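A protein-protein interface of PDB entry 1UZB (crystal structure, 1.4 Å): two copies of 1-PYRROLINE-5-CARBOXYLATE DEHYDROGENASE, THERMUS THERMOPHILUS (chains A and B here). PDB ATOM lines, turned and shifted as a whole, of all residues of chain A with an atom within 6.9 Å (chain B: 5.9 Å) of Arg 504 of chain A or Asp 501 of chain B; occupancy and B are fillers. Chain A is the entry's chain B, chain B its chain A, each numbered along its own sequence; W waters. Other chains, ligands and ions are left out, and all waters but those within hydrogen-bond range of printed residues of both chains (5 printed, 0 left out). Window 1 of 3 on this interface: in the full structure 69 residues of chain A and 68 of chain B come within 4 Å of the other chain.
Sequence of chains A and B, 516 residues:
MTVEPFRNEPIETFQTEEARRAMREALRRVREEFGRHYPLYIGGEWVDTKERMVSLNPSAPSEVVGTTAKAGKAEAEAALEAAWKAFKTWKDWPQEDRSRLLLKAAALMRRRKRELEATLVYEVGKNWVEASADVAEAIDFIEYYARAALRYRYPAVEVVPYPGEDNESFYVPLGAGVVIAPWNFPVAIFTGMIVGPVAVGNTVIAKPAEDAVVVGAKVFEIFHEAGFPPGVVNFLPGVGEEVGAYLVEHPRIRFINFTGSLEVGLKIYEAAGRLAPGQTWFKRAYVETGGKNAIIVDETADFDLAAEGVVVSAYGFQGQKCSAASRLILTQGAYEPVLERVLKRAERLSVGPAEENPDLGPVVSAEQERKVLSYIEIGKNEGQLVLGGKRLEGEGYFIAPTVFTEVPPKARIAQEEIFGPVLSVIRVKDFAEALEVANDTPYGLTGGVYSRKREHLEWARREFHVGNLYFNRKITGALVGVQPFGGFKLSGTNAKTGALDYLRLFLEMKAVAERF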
ATOM      1  N   TYR A 152      27.693 -10.115  13.816  1.00  0.00           N
ATOM      2  CA  TYR A 152      26.435 -10.626  14.357  1.00  0.00           C
ATOM      3  C   TYR A 152      25.730  -9.629  15.271  1.00  0.00           C
ATOM      4  O   TYR A 152      24.704  -9.955  15.859  1.00  0.00           O
ATOM      5  CB  TYR A 152      26.678 -11.917  15.154  1.00  0.00           C
ATOM      6  CG  TYR A 152      27.171 -13.082  14.329  1.00  0.00           C
ATOM      7  CD1 TYR A 152      28.532 -13.290  14.116  1.00  0.00           C
ATOM      8  CD2 TYR A 152      26.272 -13.965  13.742  1.00  0.00           C
ATOM      9  CE1 TYR A 152      28.982 -14.350  13.335  1.00  0.00           C
ATOM     10  CE2 TYR A 152      26.710 -15.025  12.961  1.00  0.00           C
ATOM     11  CZ  TYR A 152      28.066 -15.212  12.762  1.00  0.00           C
ATOM     12  OH  TYR A 152      28.503 -16.268  11.998  1.00  0.00           O
ATOM     13  N   VAL A 157      19.932  -9.845  11.563  1.00  0.00           N
ATOM     14  CA  VAL A 157      19.217 -10.697  10.616  1.00  0.00           C
ATOM     15  C   VAL A 157      18.446  -9.986   9.510  1.00  0.00           C
ATOM     16  O   VAL A 157      17.696  -9.044   9.758  1.00  0.00           O
ATOM     17  CB  VAL A 157      18.262 -11.641  11.364  1.00  0.00           C
ATOM     18  CG1 VAL A 157      17.659 -12.650  10.394  1.00  0.00           C
ATOM     19  CG2 VAL A 157      19.017 -12.361  12.476  1.00  0.00           C
ATOM     20  N   TYR A 171      20.466 -11.902  17.158  1.00  0.00           N
ATOM     21  CA  TYR A 171      21.094 -13.020  17.842  1.00  0.00           C
ATOM     22  C   TYR A 171      21.379 -12.731  19.304  1.00  0.00           C
ATOM     23  O   TYR A 171      21.638 -11.591  19.685  1.00  0.00           O
ATOM     24  CB  TYR A 171      22.408 -13.386  17.149  1.00  0.00           C
ATOM     25  CG  TYR A 171      22.242 -13.829  15.719  1.00  0.00           C
ATOM     26  CD1 TYR A 171      22.680 -13.029  14.666  1.00  0.00           C
ATOM     27  CD2 TYR A 171      21.638 -15.046  15.415  1.00  0.00           C
ATOM     28  CE1 TYR A 171      22.519 -13.427  13.345  1.00  0.00           C
ATOM     29  CE2 TYR A 171      21.469 -15.454  14.097  1.00  0.00           C
ATOM     30  CZ  TYR A 171      21.914 -14.639  13.068  1.00  0.00           C
ATOM     31  OH  TYR A 171      21.763 -15.029  11.757  1.00  0.00           O
ATOM     32  N   LEU A 174      23.892 -18.178  24.107  1.00  0.00           N
ATOM     33  CA  LEU A 174      23.205 -19.308  24.726  1.00  0.00           C
ATOM     34  C   LEU A 174      23.242 -19.343  26.250  1.00  0.00           C
ATOM     35  O   LEU A 174      22.219 -19.577  26.892  1.00  0.00           O
ATOM     36  CB  LEU A 174      23.792 -20.617  24.196  1.00  0.00           C
ATOM     37  CG  LEU A 174      23.833 -20.762  22.673  1.00  0.00           C
ATOM     38  CD1 LEU A 174      24.563 -22.044  22.313  1.00  0.00           C
ATOM     39  CD2 LEU A 174      22.419 -20.759  22.114  1.00  0.00           C
ATOM     40  N   VAL A 200      30.787 -13.546  21.759  1.00  0.00           N
ATOM     41  CA  VAL A 200      29.405 -13.190  21.463  1.00  0.00           C
ATOM     42  C   VAL A 200      28.456 -13.175  22.661  1.00  0.00           C
ATOM     43  O   VAL A 200      27.240 -13.062  22.495  1.00  0.00           O
ATOM     44  CB  VAL A 200      28.821 -14.093  20.343  1.00  0.00           C
ATOM     45  CG1 VAL A 200      29.587 -13.861  19.046  1.00  0.00           C
ATOM     46  CG2 VAL A 200      28.892 -15.556  20.746  1.00  0.00           C
ATOM     47  N   ARG A 284      23.763 -28.232  22.932  1.00  0.00           N
ATOM     48  CA  ARG A 284      24.500 -28.189  21.683  1.00  0.00           C
ATOM     49  C   ARG A 284      25.885 -28.717  22.025  1.00  0.00           C
ATOM     50  O   ARG A 284      26.474 -28.319  23.030  1.00  0.00           O
ATOM     51  CB  ARG A 284      24.624 -26.764  21.149  1.00  0.00           C
ATOM     52  CG  ARG A 284      23.314 -26.157  20.707  1.00  0.00           C
ATOM     53  CD  ARG A 284      23.556 -24.878  19.940  1.00  0.00           C
ATOM     54  NE  ARG A 284      22.299 -24.230  19.591  1.00  0.00           N
ATOM     55  CZ  ARG A 284      22.210 -23.082  18.932  1.00  0.00           C
ATOM     56  NH1 ARG A 284      23.308 -22.449  18.546  1.00  0.00           N
ATOM     57  NH2 ARG A 284      21.020 -22.566  18.659  1.00  0.00           N
ATOM     58  N   TYR A 286      29.650 -29.465  20.171  1.00  0.00           N
ATOM     59  CA  TYR A 286      30.498 -29.320  19.004  1.00  0.00           C
ATOM     60  C   TYR A 286      31.736 -30.147  19.284  1.00  0.00           C
ATOM     61  O   TYR A 286      32.395 -29.959  20.303  1.00  0.00           O
ATOM     62  CB  TYR A 286      30.843 -27.843  18.783  1.00  0.00           C
ATOM     63  CG  TYR A 286      29.822 -26.864  19.331  1.00  0.00           C
ATOM     64  CD1 TYR A 286      29.880 -26.436  20.656  1.00  0.00           C
ATOM     65  CD2 TYR A 286      28.794 -26.376  18.529  1.00  0.00           C
ATOM     66  CE1 TYR A 286      28.939 -25.547  21.170  1.00  0.00           C
ATOM     67  CE2 TYR A 286      27.846 -25.488  19.032  1.00  0.00           C
ATOM     68  CZ  TYR A 286      27.924 -25.076  20.352  1.00  0.00           C
ATOM     69  OH  TYR A 286      26.996 -24.190  20.854  1.00  0.00           O
ATOM     70  N   ALA A 499      36.622 -19.215  11.267  1.00  0.00           N
ATOM     71  CA  ALA A 499      35.690 -18.830  10.222  1.00  0.00           C
ATOM     72  C   ALA A 499      34.490 -18.114  10.831  1.00  0.00           C
ATOM     73  O   ALA A 499      34.139 -18.343  11.991  1.00  0.00           O
ATOM     74  CB  ALA A 499      35.229 -20.065   9.466  1.00  0.00           C
ATOM     75  N   LEU A 500      33.862 -17.254  10.036  1.00  0.00           N
ATOM     76  CA  LEU A 500      32.695 -16.497  10.479  1.00  0.00           C
ATOM     77  C   LEU A 500      31.607 -17.409  11.034  1.00  0.00           C
ATOM     78  O   LEU A 500      30.961 -17.091  12.037  1.00  0.00           O
ATOM     79  CB  LEU A 500      32.125 -15.693   9.309  1.00  0.00           C
ATOM     80  CG  LEU A 500      33.046 -14.621   8.724  1.00  0.00           C
ATOM     81  CD1 LEU A 500      32.439 -14.047   7.448  1.00  0.00           C
ATOM     82  CD2 LEU A 500      33.262 -13.530   9.758  1.00  0.00           C
ATOM     83  N   ASP A 501      31.417 -18.546  10.372  1.00  0.00           N
ATOM     84  CA  ASP A 501      30.397 -19.518  10.753  1.00  0.00           C
ATOM     85  C   ASP A 501      30.556 -20.103  12.151  1.00  0.00           C
ATOM     86  O   ASP A 501      29.585 -20.560  12.746  1.00  0.00           O
ATOM     87  CB  ASP A 501      30.367 -20.672   9.746  1.00  0.00           C
ATOM     88  CG  ASP A 501      29.625 -20.326   8.472  1.00  0.00           C
ATOM     89  OD1 ASP A 501      29.214 -19.158   8.296  1.00  0.00           O
ATOM     90  OD2 ASP A 501      29.457 -21.239   7.638  1.00  0.00           O
ATOM     91  N   TYR A 502      31.774 -20.098  12.677  1.00  0.00           N
ATOM     92  CA  TYR A 502      32.008 -20.667  13.998  1.00  0.00           C
ATOM     93  C   TYR A 502      31.176 -20.008  15.089  1.00  0.00           C
ATOM     94  O   TYR A 502      30.595 -20.688  15.927  1.00  0.00           O
ATOM     95  CB  TYR A 502      33.485 -20.545  14.364  1.00  0.00           C
ATOM     96  CG  TYR A 502      33.919 -21.352  15.571  1.00  0.00           C
ATOM     97  CD1 TYR A 502      33.901 -22.748  15.543  1.00  0.00           C
ATOM     98  CD2 TYR A 502      34.435 -20.722  16.703  1.00  0.00           C
ATOM     99  CE1 TYR A 502      34.401 -23.496  16.608  1.00  0.00           C
ATOM    100  CE2 TYR A 502      34.939 -21.461  17.773  1.00  0.00           C
ATOM    101  CZ  TYR A 502      34.922 -22.845  17.714  1.00  0.00           C
ATOM    102  OH  TYR A 502      35.481 -23.577  18.740  1.00  0.00           O
ATOM    103  N   LEU A 503      31.108 -18.682  15.072  1.00  0.00           N
ATOM    104  CA  LEU A 503      30.377 -17.971  16.115  1.00  0.00           C
ATOM    105  C   LEU A 503      28.869 -18.209  16.098  1.00  0.00           C
ATOM    106  O   LEU A 503      28.219 -18.152  17.143  1.00  0.00           O
ATOM    107  CB  LEU A 503      30.701 -16.475  16.047  1.00  0.00           C
ATOM    108  CG  LEU A 503      32.201 -16.147  16.109  1.00  0.00           C
ATOM    109  CD1 LEU A 503      32.380 -14.640  16.165  1.00  0.00           C
ATOM    110  CD2 LEU A 503      32.846 -16.801  17.332  1.00  0.00           C
ATOM    111  N   ARG A 504      28.315 -18.496  14.923  1.00  0.00           N
ATOM    112  CA  ARG A 504      26.881 -18.751  14.805  1.00  0.00           C
ATOM    113  C   ARG A 504      26.462 -19.948  15.659  1.00  0.00           C
ATOM    114  O   ARG A 504      25.319 -20.039  16.117  1.00  0.00           O
ATOM    115  CB  ARG A 504      26.520 -19.023  13.344  1.00  0.00           C
ATOM    116  CG  ARG A 504      25.040 -19.297  13.108  1.00  0.00           C
ATOM    117  CD  ARG A 504      24.202 -18.080  13.452  1.00  0.00           C
ATOM    118  NE  ARG A 504      22.772 -18.306  13.250  1.00  0.00           N
ATOM    119  CZ  ARG A 504      21.976 -18.940  14.106  1.00  0.00           C
ATOM    120  NH1 ARG A 504      20.687 -19.086  13.818  1.00  0.00           N
ATOM    121  NH2 ARG A 504      22.461 -19.423  15.243  1.00  0.00           N
ATOM    122  N   LEU A 505      27.396 -20.866  15.868  1.00  0.00           N
ATOM    123  CA  LEU A 505      27.128 -22.062  16.655  1.00  0.00           C
ATOM    124  C   LEU A 505      26.816 -21.755  18.114  1.00  0.00           C
ATOM    125  O   LEU A 505      26.178 -22.552  18.803  1.00  0.00           O
ATOM    126  CB  LEU A 505      28.336 -22.996  16.597  1.00  0.00           C
ATOM    127  CG  LEU A 505      28.797 -23.469  15.219  1.00  0.00           C
ATOM    128  CD1 LEU A 505      30.092 -24.258  15.373  1.00  0.00           C
ATOM    129  CD2 LEU A 505      27.714 -24.317  14.561  1.00  0.00           C
ATOM    130  N   PHE A 506      27.266 -20.595  18.583  1.00  0.00           N
ATOM    131  CA  PHE A 506      27.075 -20.203  19.977  1.00  0.00           C
ATOM    132  C   PHE A 506      26.039 -19.106  20.158  1.00  0.00           C
ATOM    133  O   PHE A 506      26.065 -18.359  21.144  1.00  0.00           O
ATOM    134  CB  PHE A 506      28.419 -19.767  20.558  1.00  0.00           C
ATOM    135  CG  PHE A 506      29.494 -20.801  20.374  1.00  0.00           C
ATOM    136  CD1 PHE A 506      30.306 -20.788  19.245  1.00  0.00           C
ATOM    137  CD2 PHE A 506      29.637 -21.837  21.287  1.00  0.00           C
ATOM    138  CE1 PHE A 506      31.243 -21.799  19.027  1.00  0.00           C
ATOM    139  CE2 PHE A 506      30.568 -22.851  21.077  1.00  0.00           C
ATOM    140  CZ  PHE A 506      31.371 -22.832  19.946  1.00  0.00           C
ATOM    141  N   LEU A 507      25.111 -19.036  19.209  1.00  0.00           N
ATOM    142  CA  LEU A 507      24.048 -18.040  19.226  1.00  0.00           C
ATOM    143  C   LEU A 507      22.704 -18.657  18.854  1.00  0.00           C
ATOM    144  O   LEU A 507      22.642 -19.679  18.164  1.00  0.00           O
ATOM    145  CB  LEU A 507      24.346 -16.932  18.208  1.00  0.00           C
ATOM    146  CG  LEU A 507      25.584 -16.057  18.392  1.00  0.00           C
ATOM    147  CD1 LEU A 507      25.845 -15.267  17.119  1.00  0.00           C
ATOM    148  CD2 LEU A 507      25.383 -15.129  19.581  1.00  0.00           C
ATOM    149  N   GLU A 508      21.631 -18.037  19.333  1.00  0.00           N
ATOM    150  CA  GLU A 508      20.290 -18.454  18.959  1.00  0.00           C
ATOM    151  C   GLU A 508      19.605 -17.173  18.480  1.00  0.00           C
ATOM    152  O   GLU A 508      20.066 -16.069  18.785  1.00  0.00           O
ATOM    153  CB  GLU A 508      19.546 -19.142  20.118  1.00  0.00           C
ATOM    154  CG  GLU A 508      19.428 -18.399  21.431  1.00  0.00           C
ATOM    155  CD  GLU A 508      18.984 -19.321  22.566  1.00  0.00           C
ATOM    156  OE1 GLU A 508      18.576 -20.473  22.286  1.00  0.00           O
ATOM    157  OE2 GLU A 508      19.042 -18.897  23.738  1.00  0.00           O
ATOM    158  N   MET A 509      18.537 -17.311  17.706  1.00  0.00           N
ATOM    159  CA  MET A 509      17.863 -16.145  17.149  1.00  0.00           C
ATOM    160  C   MET A 509      16.482 -15.855  17.720  1.00  0.00           C
ATOM    161  O   MET A 509      15.700 -16.768  17.992  1.00  0.00           O
ATOM    162  CB  MET A 509      17.746 -16.305  15.630  1.00  0.00           C
ATOM    163  CG  MET A 509      17.310 -15.040  14.896  1.00  0.00           C
ATOM    164  SD  MET A 509      16.641 -15.340  13.230  1.00  0.00           S
ATOM    165  CE  MET A 509      18.051 -16.088  12.395  1.00  0.00           C
ATOM    166  N   TYR B 152      23.985 -19.383  -0.953  1.00  0.00           N
ATOM    167  CA  TYR B 152      25.014 -20.328  -0.523  1.00  0.00           C
ATOM    168  C   TYR B 152      25.762 -20.956  -1.693  1.00  0.00           C
ATOM    169  O   TYR B 152      26.570 -21.864  -1.496  1.00  0.00           O
ATOM    170  CB  TYR B 152      24.389 -21.460   0.303  1.00  0.00           C
ATOM    171  CG  TYR B 152      23.787 -21.026   1.618  1.00  0.00           C
ATOM    172  CD1 TYR B 152      22.460 -20.611   1.699  1.00  0.00           C
ATOM    173  CD2 TYR B 152      24.551 -21.019   2.782  1.00  0.00           C
ATOM    174  CE1 TYR B 152      21.907 -20.195   2.912  1.00  0.00           C
ATOM    175  CE2 TYR B 152      24.012 -20.612   3.998  1.00  0.00           C
ATOM    176  CZ  TYR B 152      22.692 -20.200   4.057  1.00  0.00           C
ATOM    177  OH  TYR B 152      22.158 -19.799   5.259  1.00  0.00           O
ATOM    178  N   ASN B 494      15.920 -24.324  17.876  1.00  0.00           N
ATOM    179  CA  ASN B 494      15.983 -22.986  17.288  1.00  0.00           C
ATOM    180  C   ASN B 494      16.336 -22.982  15.803  1.00  0.00           C
ATOM    181  O   ASN B 494      17.055 -22.100  15.332  1.00  0.00           O
ATOM    182  CB  ASN B 494      16.979 -22.103  18.064  1.00  0.00           C
ATOM    183  CG  ASN B 494      16.810 -20.617  17.763  1.00  0.00           C
ATOM    184  OD1 ASN B 494      17.720 -19.967  17.251  1.00  0.00           O
ATOM    185  ND2 ASN B 494      15.638 -20.076  18.087  1.00  0.00           N
ATOM    186  N   LYS B 496      15.447 -21.857  12.758  1.00  0.00           N
ATOM    187  CA  LYS B 496      14.534 -20.832  12.271  1.00  0.00           C
ATOM    188  C   LYS B 496      14.022 -21.063  10.855  1.00  0.00           C
ATOM    189  O   LYS B 496      14.744 -20.855   9.880  1.00  0.00           O
ATOM    190  CB  LYS B 496      15.212 -19.463  12.365  1.00  0.00           C
ATOM    191  CG  LYS B 496      15.344 -18.921  13.789  1.00  0.00           C
ATOM    192  CD  LYS B 496      13.965 -18.706  14.411  1.00  0.00           C
ATOM    193  CE  LYS B 496      13.953 -17.581  15.435  1.00  0.00           C
ATOM    194  NZ  LYS B 496      12.573 -17.332  15.940  1.00  0.00           N
ATOM    195  N   ALA B 499      13.808 -18.521   7.096  1.00  0.00           N
ATOM    196  CA  ALA B 499      14.928 -17.614   7.291  1.00  0.00           C
ATOM    197  C   ALA B 499      16.152 -18.157   6.565  1.00  0.00           C
ATOM    198  O   ALA B 499      16.285 -19.368   6.369  1.00  0.00           O
ATOM    199  CB  ALA B 499      15.227 -17.469   8.776  1.00  0.00           C
ATOM    200  N   LEU B 500      17.048 -17.257   6.174  1.00  0.00           N
ATOM    201  CA  LEU B 500      18.266 -17.644   5.475  1.00  0.00           C
ATOM    202  C   LEU B 500      19.047 -18.701   6.253  1.00  0.00           C
ATOM    203  O   LEU B 500      19.570 -19.645   5.669  1.00  0.00           O
ATOM    204  CB  LEU B 500      19.149 -16.412   5.249  1.00  0.00           C
ATOM    205  CG  LEU B 500      18.553 -15.300   4.380  1.00  0.00           C
ATOM    206  CD1 LEU B 500      19.442 -14.068   4.432  1.00  0.00           C
ATOM    207  CD2 LEU B 500      18.399 -15.790   2.954  1.00  0.00           C
ATOM    208  N   ASP B 501      19.111 -18.542   7.572  1.00  0.00           N
ATOM    209  CA  ASP B 501      19.846 -19.461   8.436  1.00  0.00           C
ATOM    210  C   ASP B 501      19.368 -20.905   8.383  1.00  0.00           C
ATOM    211  O   ASP B 501      20.128 -21.820   8.680  1.00  0.00           O
ATOM    212  CB  ASP B 501      19.788 -18.991   9.896  1.00  0.00           C
ATOM    213  CG  ASP B 501      20.721 -17.833  10.181  1.00  0.00           C
ATOM    214  OD1 ASP B 501      21.390 -17.345   9.243  1.00  0.00           O
ATOM    215  OD2 ASP B 501      20.785 -17.413  11.358  1.00  0.00           O
ATOM    216  N   TYR B 502      18.111 -21.115   8.009  1.00  0.00           N
ATOM    217  CA  TYR B 502      17.577 -22.471   7.969  1.00  0.00           C
ATOM    218  C   TYR B 502      18.375 -23.396   7.059  1.00  0.00           C
ATOM    219  O   TYR B 502      18.689 -24.523   7.434  1.00  0.00           O
ATOM    220  CB  TYR B 502      16.119 -22.448   7.509  1.00  0.00           C
ATOM    221  CG  TYR B 502      15.371 -23.751   7.713  1.00  0.00           C
ATOM    222  CD1 TYR B 502      15.120 -24.238   8.995  1.00  0.00           C
ATOM    223  CD2 TYR B 502      14.839 -24.449   6.629  1.00  0.00           C
ATOM    224  CE1 TYR B 502      14.349 -25.379   9.197  1.00  0.00           C
ATOM    225  CE2 TYR B 502      14.061 -25.592   6.818  1.00  0.00           C
ATOM    226  CZ  TYR B 502      13.817 -26.044   8.106  1.00  0.00           C
ATOM    227  OH  TYR B 502      13.003 -27.137   8.305  1.00  0.00           O
ATOM    228  N   LEU B 503      18.718 -22.920   5.866  1.00  0.00           N
ATOM    229  CA  LEU B 503      19.440 -23.760   4.920  1.00  0.00           C
ATOM    230  C   LEU B 503      20.858 -24.141   5.344  1.00  0.00           C
ATOM    231  O   LEU B 503      21.360 -25.196   4.956  1.00  0.00           O
ATOM    232  CB  LEU B 503      19.453 -23.100   3.536  1.00  0.00           C
ATOM    233  CG  LEU B 503      18.067 -22.740   2.983  1.00  0.00           C
ATOM    234  CD1 LEU B 503      18.209 -22.202   1.569  1.00  0.00           C
ATOM    235  CD2 LEU B 503      17.158 -23.965   2.997  1.00  0.00           C
ATOM    236  N   ARG B 504      21.500 -23.297   6.146  1.00  0.00           N
ATOM    237  CA  ARG B 504      22.856 -23.582   6.612  1.00  0.00           C
ATOM    238  C   ARG B 504      22.896 -24.882   7.419  1.00  0.00           C
ATOM    239  O   ARG B 504      23.923 -25.562   7.477  1.00  0.00           O
ATOM    240  CB  ARG B 504      23.365 -22.428   7.483  1.00  0.00           C
ATOM    241  CG  ARG B 504      24.772 -22.634   8.041  1.00  0.00           C
ATOM    242  CD  ARG B 504      25.796 -22.648   6.926  1.00  0.00           C
ATOM    243  NE  ARG B 504      27.154 -22.893   7.403  1.00  0.00           N
ATOM    244  CZ  ARG B 504      27.632 -24.088   7.735  1.00  0.00           C
ATOM    245  NH1 ARG B 504      28.885 -24.199   8.154  1.00  0.00           N
ATOM    246  NH2 ARG B 504      26.868 -25.174   7.645  1.00  0.00           N
ATOM    247  N   LEU B 505      21.770 -25.211   8.048  1.00  0.00           N
ATOM    248  CA  LEU B 505      21.659 -26.416   8.861  1.00  0.00           C
ATOM    249  C   LEU B 505      21.804 -27.697   8.048  1.00  0.00           C
ATOM    250  O   LEU B 505      22.135 -28.755   8.590  1.00  0.00           O
ATOM    251  CB  LEU B 505      20.304 -26.433   9.566  1.00  0.00           C
ATOM    252  CG  LEU B 505      19.998 -25.259  10.497  1.00  0.00           C
ATOM    253  CD1 LEU B 505      18.552 -25.349  10.948  1.00  0.00           C
ATOM    254  CD2 LEU B 505      20.943 -25.272  11.683  1.00  0.00           C
HETATM  255  O   HOH W   1      24.188 -16.596  10.368  1.00  0.00           O
HETATM  256  O   HOH W   2      20.895 -14.575   9.214  1.00  0.00           O
HETATM  257  O   HOH W   3      20.117 -20.935  16.339  1.00  0.00           O
HETATM  258  O   HOH W   4      18.199 -20.867  13.067  1.00  0.00           O
HETATM  259  O   HOH W   5      20.270 -21.944  11.851  1.00  0.00           O
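OH of Tyr 171 of chain A is in hydrogen-bond range of OD2 of Asp 501 of chain B (2.6 Å). The backbone NH of Met 509 of chain A is in hydrogen-bond range of the side-chain amide oxygen of Asn 494 of chain B, at 2.8 Å. OD2 of Asp 501 of chain A lies within salt-bridge range of NE of Arg 504 of chain B. The side-chain carboxylate (OD2) of Asp 501 of chain B lies within salt-bridge range of the guanidinium group (NE) of Arg 504 of chain A, 2.9 Å away.
The guanidinium group of Arg 504 of chain A sits at hydrogen-bond distance from the backbone carbonyl oxygen of Leu 507 of chain A.
Among the printed residues, pairs that only touch across the chains: Met 509 of chain A with Lys 496 of chain B, Met 509 of chain A with Asp 501 of chain B and Glu 508 of chain A with Asn 494 of chain B.
Of chain B, only Asp 501 comes within 4 Å of Arg 504 of chain A. Of chain A, only Tyr 171, Arg 504 and Met 509 come within 4 Å of Asp 501 of chain B. Of the printed residues of chain B, Met 509 of chain A touches Asn 494 (2.8 Å), Lys 496 (3.2 Å) and Asp 501 (3.2 Å). Printed residues of chain B within 4 Å of Glu 508 of chain A: Asn 494. Leu 500 of chain A touches none of the printed residues of chain B. Leu 505 of chain B touches none of the printed residues of chain A.
Of the 10 printed residues of chain B, 4 touch a printed residue of chain A. Printed residues of chain B that touch a printed residue of chain A: Asn 494, Lys 496, Asp 501 and Arg 504. Of the 18 printed residues of chain A, 5 touch a printed residue of chain B. Hydrophobic or aromatic side chains of chain A within 4 Å of the printed part of chain B: Tyr 171 and Met 509.
Asp 501 of chain A touches Arg 504 of chain B, and with the chains exchanged Arg 504 of chain A touches Asp 501 of chain B. Positions printed for both chains: 152, 499, 500, 501, 502, 503, 504 and 505. Of the 7 pairs that touch across the chains among the printed residues, 2 have their exchanged pair printed and touching as well.
Water W2 bridges the side-chain hydroxyl of Tyr 171 of chain A (2.7 Å) and the side-chain carboxylate of Asp 501 of chain B (2.8 Å). Water W3 lies within hydrogen-bond range of OD1 of Asn 494 of chain B, NH2 of Arg 284 of chain A, NH2 of Arg 504 of chain A and O of Leu 507 of chain A. Water W4 lies within hydrogen-bond range of the backbone carbonyl oxygen of Asn 494 of chain B (2.8 Å), the backbone NH of Lys 496 of chain B (2.9 Å) and the guanidinium group of Arg 504 of chain A (3.2 Å). Water W1 bridges the side-chain carboxylate of Asp 501 of chain B and the side-chain hydroxyl of Tyr 171 of chain A. Water W5 bridges the backbone carbonyl oxygen of Asp 501 of chain B (3.2 Å) and the guanidinium group of Arg 504 of chain A (3.5 Å).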
